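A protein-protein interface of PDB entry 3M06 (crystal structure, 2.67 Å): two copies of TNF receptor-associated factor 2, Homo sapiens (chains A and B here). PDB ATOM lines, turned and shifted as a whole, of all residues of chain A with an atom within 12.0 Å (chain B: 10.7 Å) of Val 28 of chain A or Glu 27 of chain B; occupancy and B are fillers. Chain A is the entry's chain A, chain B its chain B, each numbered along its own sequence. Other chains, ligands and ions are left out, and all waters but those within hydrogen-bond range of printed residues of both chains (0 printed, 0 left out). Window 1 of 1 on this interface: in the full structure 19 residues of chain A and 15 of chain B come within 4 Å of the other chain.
OG1 of Thr 34 of chain B sits at hydrogen-bond distance from O of Arg 30 of chain B (3.2 Å).
The backbone carbonyl oxygen (O) of Glu 18 of chain A is in hydrogen-bond range of the side-chain sulfur (SG) of Cys 22 of chain A.
O of Cys 22 of chain A sits close to OD1 of Asn 25 of chain A (2.8 Å).
The side-chain amide nitrogen (ND2) of Asn 25 of chain A is in hydrogen-bond range of the side-chain carboxylate (OE2) of Glu 29 of chain A.
Among the printed residues, merely in contact across the chains: Phe 17 of chain A with Phe 17 of chain B, Phe 17 of chain A with Val 21 of chain B, Glu 18 of chain A with Phe 17 of chain B, Val 21 of chain A with Ile 20 of chain B, Asn 25 of chain A with Leu 24 of chain B, Val 28 of chain A with Glu 27 of chain B, Val 31 of chain A with Val 31 of chain B, Ala 32 of chain A with Val 31 of chain B and Ala 35 of chain A with Thr 34 of chain B.
Printed residues of chain B within 4 Å of Val 21 of chain A: Ile 20.
No residue of chain B comes within 4 Å of Glu 27 of chain A.
Of chain B, only Glu 27 (3.5 Å) comes within 4 Å of Val 28 of chain A.
No residue of chain B comes within 4 Å of Glu 29 of chain A.
Of chain B, only Val 31 comes within 4 Å of Val 31 of chain A.
Of the printed residues of chain B, Ala 32 of chain A touches Val 31.
Of the printed residues of chain B, Ala 35 of chain A touches Thr 34 (3.5 Å).
Printed residues of chain A within 4 Å of Phe 17 of chain B: Phe 17 and Glu 18.
Asn 19 of chain B touches none of the printed residues of chain A.
No residue of chain A comes within 4 Å of Val 23 of chain B.
Of chain A, only Asn 25 (3.7 Å) comes within 4 Å of Leu 24 of chain B.
No residue of chain A comes within 4 Å of Asn 25 of chain B.
Of the printed residues of chain A, Glu 27 of chain B touches Val 28 (3.5 Å).
No residue of chain A comes within 4 Å of Val 28 of chain B.
No residue of chain A comes within 4 Å of Glu 29 of chain B.
No residue of chain A comes within 4 Å of Arg 30 of chain B.
Val 31 of chain B touches just these residues of chain A: Val 31 (3.7 Å) and Ala 32 (3.5 Å).
Printed residues of chain A that touch a printed residue of chain B: Phe 17, Glu 18, Val 21, Asn 25, Val 28, Val 31, Ala 32 and Ala 35.
Hydrophobic or aromatic side chains of chain A that line the printed part of chain B: Phe 17, Val 21, Val 28, Val 31, Ala 32 and Ala 35.
Hydrophobic or aromatic side chains of chain B that line the printed part of chain A: Phe 17, Ile 20, Val 21, Leu 24 and Val 31.
Among the printed residues, no Asp or Glu carboxylate lies within 4 Å of a Lys or Arg side-chain nitrogen of the other chain.
Val 21 of chain A touches Ile 20 of chain B, but with the chains exchanged Ile 20 of chain A does not touch Val 21 of chain B (8.9 Å).
Asn 25 of chain A touches Leu 24 of chain B, but with the chains exchanged Leu 24 of chain A does not touch Asn 25 of chain B (8.3 Å).
Val 28 of chain A touches Glu 27 of chain B, but with the chains exchanged Glu 27 of chain A does not touch Val 28 of chain B (8.7 Å).
Ala 32 of chain A touches Val 31 of chain B, but with the chains exchanged Val 31 of chain A does not touch Ala 32 of chain B (6.9 Å).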
ATOM      1  N   PHE A  17      20.414  -8.125  31.048  1.00  0.00           N
ATOM      2  CA  PHE A  17      20.490  -9.135  30.000  1.00  0.00           C
ATOM      3  C   PHE A  17      19.810  -8.738  28.692  1.00  0.00           C
ATOM      4  O   PHE A  17      20.356  -8.954  27.612  1.00  0.00           O
ATOM      5  CB  PHE A  17      19.865 -10.446  30.478  1.00  0.00           C
ATOM      6  CG  PHE A  17      19.601 -11.413  29.367  1.00  0.00           C
ATOM      7  CD1 PHE A  17      18.452 -11.304  28.596  1.00  0.00           C
ATOM      8  CD2 PHE A  17      20.512 -12.422  29.075  1.00  0.00           C
ATOM      9  CE1 PHE A  17      18.203 -12.197  27.546  1.00  0.00           C
ATOM     10  CE2 PHE A  17      20.275 -13.321  28.040  1.00  0.00           C
ATOM     11  CZ  PHE A  17      19.113 -13.208  27.271  1.00  0.00           C
ATOM     12  N   GLU A  18      18.600  -8.198  28.785  1.00  0.00           N
ATOM     13  CA  GLU A  18      17.880  -7.777  27.589  1.00  0.00           C
ATOM     14  C   GLU A  18      18.653  -6.702  26.852  1.00  0.00           C
ATOM     15  O   GLU A  18      18.843  -6.799  25.663  1.00  0.00           O
ATOM     16  CB  GLU A  18      16.496  -7.250  27.938  1.00  0.00           C
ATOM     17  CG  GLU A  18      15.579  -8.265  28.559  1.00  0.00           C
ATOM     18  CD  GLU A  18      14.457  -7.600  29.355  1.00  0.00           C
ATOM     19  OE1 GLU A  18      14.683  -7.327  30.558  1.00  0.00           O
ATOM     20  OE2 GLU A  18      13.374  -7.311  28.779  1.00  0.00           O
ATOM     21  N   ASN A  19      19.095  -5.672  27.559  1.00  0.00           N
ATOM     22  CA  ASN A  19      19.840  -4.600  26.915  1.00  0.00           C
ATOM     23  C   ASN A  19      21.108  -5.119  26.247  1.00  0.00           C
ATOM     24  O   ASN A  19      21.385  -4.798  25.086  1.00  0.00           O
ATOM     25  CB  ASN A  19      20.165  -3.456  27.891  1.00  0.00           C
ATOM     26  CG  ASN A  19      18.940  -2.625  28.249  1.00  0.00           C
ATOM     27  OD1 ASN A  19      18.687  -1.572  27.646  1.00  0.00           O
ATOM     28  ND2 ASN A  19      18.170  -3.094  29.233  1.00  0.00           N
ATOM     29  N   ILE A  20      21.867  -5.922  26.995  1.00  0.00           N
ATOM     30  CA  ILE A  20      23.071  -6.567  26.494  1.00  0.00           C
ATOM     31  C   ILE A  20      22.808  -7.256  25.169  1.00  0.00           C
ATOM     32  O   ILE A  20      23.622  -7.151  24.260  1.00  0.00           O
ATOM     33  CB  ILE A  20      23.616  -7.614  27.482  1.00  0.00           C
ATOM     34  CG1 ILE A  20      23.985  -6.983  28.840  1.00  0.00           C
ATOM     35  CG2 ILE A  20      24.807  -8.343  26.881  1.00  0.00           C
ATOM     36  CD1 ILE A  20      24.633  -5.613  28.767  1.00  0.00           C
ATOM     37  N   VAL A  21      21.674  -7.940  25.035  1.00  0.00           N
ATOM     38  CA  VAL A  21      21.358  -8.594  23.766  1.00  0.00           C
ATOM     39  C   VAL A  21      20.976  -7.632  22.637  1.00  0.00           C
ATOM     40  O   VAL A  21      21.390  -7.852  21.484  1.00  0.00           O
ATOM     41  CB  VAL A  21      20.296  -9.724  23.908  1.00  0.00           C
ATOM     42  CG1 VAL A  21      19.730 -10.090  22.555  1.00  0.00           C
ATOM     43  CG2 VAL A  21      20.900 -10.942  24.579  1.00  0.00           C
ATOM     44  N   CYS A  22      20.209  -6.578  22.961  1.00  0.00           N
ATOM     45  CA  CYS A  22      19.891  -5.506  22.003  1.00  0.00           C
ATOM     46  C   CYS A  22      21.149  -4.794  21.493  1.00  0.00           C
ATOM     47  O   CYS A  22      21.219  -4.416  20.309  1.00  0.00           O
ATOM     48  CB  CYS A  22      18.946  -4.469  22.606  1.00  0.00           C
ATOM     49  SG  CYS A  22      17.398  -5.155  23.214  1.00  0.00           S
ATOM     50  N   VAL A  23      22.143  -4.621  22.372  1.00  0.00           N
ATOM     51  CA  VAL A  23      23.423  -4.080  21.925  1.00  0.00           C
ATOM     52  C   VAL A  23      24.100  -5.072  20.967  1.00  0.00           C
ATOM     53  O   VAL A  23      24.358  -4.760  19.805  1.00  0.00           O
ATOM     54  CB  VAL A  23      24.377  -3.725  23.093  1.00  0.00           C
ATOM     55  CG1 VAL A  23      25.661  -3.150  22.534  1.00  0.00           C
ATOM     56  CG2 VAL A  23      23.732  -2.755  24.057  1.00  0.00           C
ATOM     57  N   LEU A  24      24.361  -6.278  21.462  1.00  0.00           N
ATOM     58  CA  LEU A  24      24.845  -7.367  20.617  1.00  0.00           C
ATOM     59  C   LEU A  24      24.131  -7.542  19.267  1.00  0.00           C
ATOM     60  O   LEU A  24      24.781  -7.838  18.275  1.00  0.00           O
ATOM     61  CB  LEU A  24      24.813  -8.675  21.401  1.00  0.00           C
ATOM     62  CG  LEU A  24      25.997  -8.683  22.354  1.00  0.00           C
ATOM     63  CD1 LEU A  24      26.209 -10.068  22.960  1.00  0.00           C
ATOM     64  CD2 LEU A  24      27.239  -8.232  21.609  1.00  0.00           C
ATOM     65  N   ASN A  25      22.812  -7.370  19.223  1.00  0.00           N
ATOM     66  CA  ASN A  25      22.107  -7.560  17.957  1.00  0.00           C
ATOM     67  C   ASN A  25      22.402  -6.458  16.930  1.00  0.00           C
ATOM     68  O   ASN A  25      22.701  -6.744  15.773  1.00  0.00           O
ATOM     69  CB  ASN A  25      20.612  -7.743  18.154  1.00  0.00           C
ATOM     70  CG  ASN A  25      19.827  -6.478  17.816  1.00  0.00           C
ATOM     71  OD1 ASN A  25      19.347  -5.752  18.712  1.00  0.00           O
ATOM     72  ND2 ASN A  25      19.682  -6.207  16.519  1.00  0.00           N
ATOM     73  N   ARG A  26      22.336  -5.201  17.354  1.00  0.00           N
ATOM     74  CA  ARG A  26      22.723  -4.064  16.499  1.00  0.00           C
ATOM     75  C   ARG A  26      24.177  -4.146  16.088  1.00  0.00           C
ATOM     76  O   ARG A  26      24.519  -3.774  14.962  1.00  0.00           O
ATOM     77  CB  ARG A  26      22.470  -2.719  17.203  1.00  0.00           C
ATOM     78  N   GLU A  27      25.035  -4.607  16.998  1.00  0.00           N
ATOM     79  CA  GLU A  27      26.444  -4.716  16.661  1.00  0.00           C
ATOM     80  C   GLU A  27      26.690  -5.802  15.635  1.00  0.00           C
ATOM     81  O   GLU A  27      27.625  -5.710  14.862  1.00  0.00           O
ATOM     82  CB  GLU A  27      27.349  -4.953  17.869  1.00  0.00           C
ATOM     83  CG  GLU A  27      28.792  -5.085  17.404  1.00  0.00           C
ATOM     84  CD  GLU A  27      29.783  -5.403  18.513  1.00  0.00           C
ATOM     85  OE1 GLU A  27      29.360  -5.548  19.694  1.00  0.00           O
ATOM     86  OE2 GLU A  27      30.999  -5.510  18.207  1.00  0.00           O
ATOM     87  N   VAL A  28      25.871  -6.847  15.642  1.00  0.00           N
ATOM     88  CA  VAL A  28      25.976  -7.897  14.631  1.00  0.00           C
ATOM     89  C   VAL A  28      25.489  -7.357  13.280  1.00  0.00           C
ATOM     90  O   VAL A  28      26.207  -7.427  12.276  1.00  0.00           O
ATOM     91  CB  VAL A  28      25.211  -9.177  15.027  1.00  0.00           C
ATOM     92  CG1 VAL A  28      25.251 -10.186  13.903  1.00  0.00           C
ATOM     93  CG2 VAL A  28      25.825  -9.797  16.253  1.00  0.00           C
ATOM     94  N   GLU A  29      24.280  -6.806  13.274  1.00  0.00           N
ATOM     95  CA  GLU A  29      23.740  -6.124  12.104  1.00  0.00           C
ATOM     96  C   GLU A  29      24.814  -5.289  11.434  1.00  0.00           C
ATOM     97  O   GLU A  29      24.926  -5.275  10.203  1.00  0.00           O
ATOM     98  CB  GLU A  29      22.596  -5.199  12.509  1.00  0.00           C
ATOM     99  CG  GLU A  29      21.414  -5.898  13.147  1.00  0.00           C
ATOM    100  CD  GLU A  29      20.438  -4.914  13.805  1.00  0.00           C
ATOM    101  OE1 GLU A  29      20.877  -3.809  14.223  1.00  0.00           O
ATOM    102  OE2 GLU A  29      19.231  -5.252  13.902  1.00  0.00           O
ATOM    103  N   ARG A  30      25.590  -4.588  12.259  1.00  0.00           N
ATOM    104  CA  ARG A  30      26.634  -3.687  11.810  1.00  0.00           C
ATOM    105  C   ARG A  30      27.865  -4.433  11.297  1.00  0.00           C
ATOM    106  O   ARG A  30      28.462  -4.044  10.280  1.00  0.00           O
ATOM    107  CB  ARG A  30      27.002  -2.716  12.936  1.00  0.00           C
ATOM    108  CG  ARG A  30      28.347  -2.031  12.804  1.00  0.00           C
ATOM    109  CD  ARG A  30      29.504  -2.928  13.259  1.00  0.00           C
ATOM    110  NE  ARG A  30      29.764  -2.868  14.694  1.00  0.00           N
ATOM    111  CZ  ARG A  30      30.716  -2.121  15.255  1.00  0.00           C
ATOM    112  NH1 ARG A  30      31.512  -1.365  14.498  1.00  0.00           N
ATOM    113  NH2 ARG A  30      30.877  -2.132  16.578  1.00  0.00           N
ATOM    114  N   VAL A  31      28.269  -5.498  11.980  1.00  0.00           N
ATOM    115  CA  VAL A  31      29.424  -6.242  11.498  1.00  0.00           C
ATOM    116  C   VAL A  31      29.104  -6.923  10.161  1.00  0.00           C
ATOM    117  O   VAL A  31      29.891  -6.848   9.227  1.00  0.00           O
ATOM    118  CB  VAL A  31      29.916  -7.319  12.502  1.00  0.00           C
ATOM    119  CG1 VAL A  31      31.038  -8.135  11.869  1.00  0.00           C
ATOM    120  CG2 VAL A  31      30.363  -6.699  13.806  1.00  0.00           C
ATOM    121  N   ALA A  32      27.944  -7.569  10.072  1.00  0.00           N
ATOM    122  CA  ALA A  32      27.513  -8.197   8.829  1.00  0.00           C
ATOM    123  C   ALA A  32      27.601  -7.227   7.650  1.00  0.00           C
ATOM    124  O   ALA A  32      27.866  -7.634   6.519  1.00  0.00           O
ATOM    125  CB  ALA A  32      26.099  -8.758   8.969  1.00  0.00           C
ATOM    126  N   MET A  33      27.371  -5.943   7.928  1.00  0.00           N
ATOM    127  CA  MET A  33      27.515  -4.881   6.940  1.00  0.00           C
ATOM    128  C   MET A  33      28.975  -4.753   6.517  1.00  0.00           C
ATOM    129  O   MET A  33      29.288  -4.672   5.332  1.00  0.00           O
ATOM    130  CB  MET A  33      27.046  -3.552   7.543  1.00  0.00           C
ATOM    131  N   THR A  34      29.853  -4.720   7.512  1.00  0.00           N
ATOM    132  CA  THR A  34      31.279  -4.546   7.304  1.00  0.00           C
ATOM    133  C   THR A  34      31.863  -5.740   6.582  1.00  0.00           C
ATOM    134  O   THR A  34      32.888  -5.615   5.895  1.00  0.00           O
ATOM    135  CB  THR A  34      32.026  -4.392   8.657  1.00  0.00           C
ATOM    136  OG1 THR A  34      31.610  -3.184   9.313  1.00  0.00           O
ATOM    137  CG2 THR A  34      33.520  -4.361   8.451  1.00  0.00           C
ATOM    138  N   ALA A  35      31.231  -6.902   6.756  1.00  0.00           N
ATOM    139  CA  ALA A  35      31.678  -8.104   6.052  1.00  0.00           C
ATOM    140  C   ALA A  35      31.098  -8.170   4.624  1.00  0.00           C
ATOM    141  O   ALA A  35      31.677  -8.791   3.725  1.00  0.00           O
ATOM    142  CB  ALA A  35      31.337  -9.361   6.848  1.00  0.00           C
ATOM    143  N   GLU A  36      29.959  -7.517   4.418  1.00  0.00           N
ATOM    144  CA  GLU A  36      29.388  -7.434   3.083  1.00  0.00           C
ATOM    145  C   GLU A  36      30.064  -6.352   2.231  1.00  0.00           C
ATOM    146  O   GLU A  36      29.958  -6.383   1.010  1.00  0.00           O
ATOM    147  CB  GLU A  36      27.873  -7.206   3.134  1.00  0.00           C
ATOM    148  N   ALA A  37      30.750  -5.397   2.861  1.00  0.00           N
ATOM    149  CA  ALA A  37      31.456  -4.348   2.115  1.00  0.00           C
ATOM    150  C   ALA A  37      32.794  -4.911   1.640  1.00  0.00           C
ATOM    151  O   ALA A  37      33.283  -4.586   0.552  1.00  0.00           O
ATOM    152  CB  ALA A  37      31.649  -3.088   2.976  1.00  0.00           C
ATOM    153  N   PHE B  17      13.220 -15.316  25.711  1.00  0.00           N
ATOM    154  CA  PHE B  17      14.677 -15.302  25.489  1.00  0.00           C
ATOM    155  C   PHE B  17      15.295 -16.584  24.930  1.00  0.00           C
ATOM    156  O   PHE B  17      16.356 -16.521  24.323  1.00  0.00           O
ATOM    157  CB  PHE B  17      15.445 -14.899  26.743  1.00  0.00           C
ATOM    158  CG  PHE B  17      15.050 -13.560  27.285  1.00  0.00           C
ATOM    159  CD1 PHE B  17      14.896 -12.472  26.438  1.00  0.00           C
ATOM    160  CD2 PHE B  17      14.837 -13.381  28.643  1.00  0.00           C
ATOM    161  CE1 PHE B  17      14.531 -11.231  26.938  1.00  0.00           C
ATOM    162  CE2 PHE B  17      14.469 -12.149  29.142  1.00  0.00           C
ATOM    163  CZ  PHE B  17      14.318 -11.077  28.283  1.00  0.00           C
ATOM    164  N   ASN B  19      14.444 -18.267  22.308  1.00  0.00           N
ATOM    165  CA  ASN B  19      14.556 -18.066  20.868  1.00  0.00           C
ATOM    166  C   ASN B  19      15.208 -16.741  20.474  1.00  0.00           C
ATOM    167  O   ASN B  19      15.662 -16.583  19.350  1.00  0.00           O
ATOM    168  CB  ASN B  19      13.203 -18.218  20.175  1.00  0.00           C
ATOM    169  CG  ASN B  19      13.338 -18.381  18.667  1.00  0.00           C
ATOM    170  OD1 ASN B  19      13.402 -19.503  18.138  1.00  0.00           O
ATOM    171  ND2 ASN B  19      13.385 -17.255  17.964  1.00  0.00           N
ATOM    172  N   ILE B  20      15.266 -15.785  21.393  1.00  0.00           N
ATOM    173  CA  ILE B  20      16.040 -14.593  21.120  1.00  0.00           C
ATOM    174  C   ILE B  20      17.503 -14.968  21.075  1.00  0.00           C
ATOM    175  O   ILE B  20      18.235 -14.490  20.211  1.00  0.00           O
ATOM    176  CB  ILE B  20      15.765 -13.482  22.161  1.00  0.00           C
ATOM    177  CG1 ILE B  20      14.423 -12.819  21.838  1.00  0.00           C
ATOM    178  CG2 ILE B  20      16.881 -12.407  22.161  1.00  0.00           C
ATOM    179  CD1 ILE B  20      13.841 -12.002  22.973  1.00  0.00           C
ATOM    180  N   VAL B  21      17.927 -15.841  21.990  1.00  0.00           N
ATOM    181  CA  VAL B  21      19.332 -16.252  22.026  1.00  0.00           C
ATOM    182  C   VAL B  21      19.676 -17.230  20.919  1.00  0.00           C
ATOM    183  O   VAL B  21      20.781 -17.196  20.383  1.00  0.00           O
ATOM    184  CB  VAL B  21      19.790 -16.774  23.403  1.00  0.00           C
ATOM    185  CG1 VAL B  21      19.802 -15.648  24.413  1.00  0.00           C
ATOM    186  CG2 VAL B  21      18.918 -17.883  23.883  1.00  0.00           C
ATOM    187  N   CYS B  22      18.719 -18.091  20.576  1.00  0.00           N
ATOM    188  CA  CYS B  22      18.852 -18.948  19.405  1.00  0.00           C
ATOM    189  C   CYS B  22      19.100 -18.100  18.154  1.00  0.00           C
ATOM    190  O   CYS B  22      19.936 -18.431  17.317  1.00  0.00           O
ATOM    191  CB  CYS B  22      17.602 -19.805  19.235  1.00  0.00           C
ATOM    192  SG  CYS B  22      17.562 -20.848  17.755  1.00  0.00           S
ATOM    193  N   VAL B  23      18.389 -16.982  18.033  1.00  0.00           N
ATOM    194  CA  VAL B  23      18.606 -16.097  16.903  1.00  0.00           C
ATOM    195  C   VAL B  23      19.959 -15.421  16.949  1.00  0.00           C
ATOM    196  O   VAL B  23      20.675 -15.378  15.941  1.00  0.00           O
ATOM    197  CB  VAL B  23      17.568 -14.988  16.788  1.00  0.00           C
ATOM    198  CG1 VAL B  23      17.873 -14.167  15.534  1.00  0.00           C
ATOM    199  CG2 VAL B  23      16.132 -15.558  16.717  1.00  0.00           C
ATOM    200  N   LEU B  24      20.311 -14.884  18.113  1.00  0.00           N
ATOM    201  CA  LEU B  24      21.476 -14.019  18.186  1.00  0.00           C
ATOM    202  C   LEU B  24      22.697 -14.833  17.830  1.00  0.00           C
ATOM    203  O   LEU B  24      23.610 -14.337  17.172  1.00  0.00           O
ATOM    204  CB  LEU B  24      21.630 -13.412  19.578  1.00  0.00           C
ATOM    205  CG  LEU B  24      22.537 -12.184  19.667  1.00  0.00           C
ATOM    206  CD1 LEU B  24      23.987 -12.568  19.674  1.00  0.00           C
ATOM    207  CD2 LEU B  24      22.247 -11.224  18.530  1.00  0.00           C
ATOM    208  N   ASN B  25      22.695 -16.085  18.290  1.00  0.00           N
ATOM    209  CA  ASN B  25      23.746 -17.056  18.036  1.00  0.00           C
ATOM    210  C   ASN B  25      23.827 -17.468  16.568  1.00  0.00           C
ATOM    211  O   ASN B  25      24.907 -17.558  15.984  1.00  0.00           O
ATOM    212  CB  ASN B  25      23.484 -18.292  18.882  1.00  0.00           C
ATOM    213  CG  ASN B  25      24.372 -19.460  18.504  1.00  0.00           C
ATOM    214  OD1 ASN B  25      24.037 -20.287  17.624  1.00  0.00           O
ATOM    215  ND2 ASN B  25      25.518 -19.549  19.183  1.00  0.00           N
ATOM    216  N   ARG B  26      22.672 -17.776  15.993  1.00  0.00           N
ATOM    217  CA  ARG B  26      22.582 -18.062  14.571  1.00  0.00           C
ATOM    218  C   ARG B  26      23.284 -16.930  13.770  1.00  0.00           C
ATOM    219  O   ARG B  26      24.192 -17.206  12.975  1.00  0.00           O
ATOM    220  CB  ARG B  26      21.107 -18.210  14.188  1.00  0.00           C
ATOM    221  CG  ARG B  26      20.801 -18.281  12.686  1.00  0.00           C
ATOM    222  CD  ARG B  26      21.107 -19.652  12.144  1.00  0.00           C
ATOM    223  NE  ARG B  26      20.624 -20.710  13.026  1.00  0.00           N
ATOM    224  CZ  ARG B  26      20.998 -21.991  12.946  1.00  0.00           C
ATOM    225  NH1 ARG B  26      21.879 -22.374  12.021  1.00  0.00           N
ATOM    226  NH2 ARG B  26      20.501 -22.895  13.797  1.00  0.00           N
ATOM    227  N   GLU B  27      22.870 -15.676  14.037  1.00  0.00           N
ATOM    228  CA  GLU B  27      23.402 -14.429  13.448  1.00  0.00           C
ATOM    229  C   GLU B  27      24.918 -14.354  13.489  1.00  0.00           C
ATOM    230  O   GLU B  27      25.562 -13.998  12.500  1.00  0.00           O
ATOM    231  CB  GLU B  27      22.914 -13.194  14.233  1.00  0.00           C
ATOM    232  CG  GLU B  27      21.423 -12.831  14.223  1.00  0.00           C
ATOM    233  CD  GLU B  27      21.153 -11.553  15.065  1.00  0.00           C
ATOM    234  OE1 GLU B  27      22.031 -10.644  15.069  1.00  0.00           O
ATOM    235  OE2 GLU B  27      20.090 -11.450  15.739  1.00  0.00           O
ATOM    236  N   VAL B  28      25.477 -14.632  14.665  1.00  0.00           N
ATOM    237  CA  VAL B  28      26.907 -14.480  14.921  1.00  0.00           C
ATOM    238  C   VAL B  28      27.669 -15.608  14.242  1.00  0.00           C
ATOM    239  O   VAL B  28      28.721 -15.376  13.637  1.00  0.00           O
ATOM    240  CB  VAL B  28      27.218 -14.469  16.442  1.00  0.00           C
ATOM    241  CG1 VAL B  28      26.785 -15.758  17.059  1.00  0.00           C
ATOM    242  CG2 VAL B  28      28.690 -14.247  16.709  1.00  0.00           C
ATOM    243  N   GLU B  29      27.125 -16.822  14.324  1.00  0.00           N
ATOM    244  CA  GLU B  29      27.669 -17.952  13.607  1.00  0.00           C
ATOM    245  C   GLU B  29      27.889 -17.538  12.148  1.00  0.00           C
ATOM    246  O   GLU B  29      28.978 -17.738  11.588  1.00  0.00           O
ATOM    247  CB  GLU B  29      26.710 -19.131  13.689  1.00  0.00           C
ATOM    248  CG  GLU B  29      26.742 -19.884  14.986  1.00  0.00           C
ATOM    249  CD  GLU B  29      25.699 -21.006  15.021  1.00  0.00           C
ATOM    250  OE1 GLU B  29      24.930 -21.127  14.033  1.00  0.00           O
ATOM    251  OE2 GLU B  29      25.631 -21.752  16.030  1.00  0.00           O
ATOM    252  N   ARG B  30      26.854 -16.949  11.544  1.00  0.00           N
ATOM    253  CA  ARG B  30      26.925 -16.504  10.146  1.00  0.00           C
ATOM    254  C   ARG B  30      27.882 -15.355   9.913  1.00  0.00           C
ATOM    255  O   ARG B  30      28.420 -15.222   8.833  1.00  0.00           O
ATOM    256  CB  ARG B  30      25.549 -16.100   9.626  1.00  0.00           C
ATOM    257  CG  ARG B  30      24.541 -17.185   9.759  1.00  0.00           C
ATOM    258  CD  ARG B  30      23.172 -16.672   9.472  1.00  0.00           C
ATOM    259  NE  ARG B  30      22.223 -17.774   9.517  1.00  0.00           N
ATOM    260  CZ  ARG B  30      20.950 -17.663   9.166  1.00  0.00           C
ATOM    261  NH1 ARG B  30      20.482 -16.491   8.744  1.00  0.00           N
ATOM    262  NH2 ARG B  30      20.153 -18.723   9.234  1.00  0.00           N
ATOM    263  N   VAL B  31      28.090 -14.505  10.907  1.00  0.00           N
ATOM    264  CA  VAL B  31      29.048 -13.420  10.716  1.00  0.00           C
ATOM    265  C   VAL B  31      30.459 -13.879  11.045  1.00  0.00           C
ATOM    266  O   VAL B  31      31.414 -13.186  10.747  1.00  0.00           O
ATOM    267  CB  VAL B  31      28.710 -12.152  11.529  1.00  0.00           C
ATOM    268  CG1 VAL B  31      29.606 -12.050  12.768  1.00  0.00           C
ATOM    269  CG2 VAL B  31      28.875 -10.917  10.672  1.00  0.00           C
ATOM    270  N   ALA B  32      30.590 -15.042  11.671  1.00  0.00           N
ATOM    271  CA  ALA B  32      31.909 -15.584  11.979  1.00  0.00           C
ATOM    272  C   ALA B  32      32.408 -16.265  10.721  1.00  0.00           C
ATOM    273  O   ALA B  32      33.562 -16.662  10.602  1.00  0.00           O
ATOM    274  CB  ALA B  32      31.815 -16.573  13.101  1.00  0.00           C
ATOM    275  N   MET B  33      31.494 -16.378   9.772  1.00  0.00           N
ATOM    276  CA  MET B  33      31.703 -17.163   8.580  1.00  0.00           C
ATOM    277  C   MET B  33      32.191 -16.214   7.508  1.00  0.00           C
ATOM    278  O   MET B  33      33.241 -16.394   6.912  1.00  0.00           O
ATOM    279  CB  MET B  33      30.366 -17.764   8.149  1.00  0.00           C
ATOM    280  CG  MET B  33      30.475 -19.091   7.485  1.00  0.00           C
ATOM    281  SD  MET B  33      31.460 -20.193   8.472  1.00  0.00           S
ATOM    282  CE  MET B  33      30.234 -21.196   9.339  1.00  0.00           C
ATOM    283  N   THR B  34      31.383 -15.197   7.268  1.00  0.00           N
ATOM    284  CA  THR B  34      31.676 -14.208   6.262  1.00  0.00           C
ATOM    285  C   THR B  34      33.004 -13.558   6.573  1.00  0.00           C
ATOM    286  O   THR B  34      33.783 -13.323   5.679  1.00  0.00           O
ATOM    287  CB  THR B  34      30.593 -13.157   6.190  1.00  0.00           C
ATOM    288  OG1 THR B  34      29.314 -13.793   6.110  1.00  0.00           O
ATOM    289  CG2 THR B  34      30.790 -12.280   4.962  1.00  0.00           C
ATOM    290  N   ALA B  35      33.284 -13.284   7.837  1.00  0.00           N
ATOM    291  CA  ALA B  35      34.552 -12.643   8.178  1.00  0.00           C
ATOM    292  C   ALA B  35      35.720 -13.643   8.164  1.00  0.00           C
ATOM    293  O   ALA B  35      36.890 -13.259   8.209  1.00  0.00           O
ATOM    294  CB  ALA B  35      34.452 -11.924   9.517  1.00  0.00           C
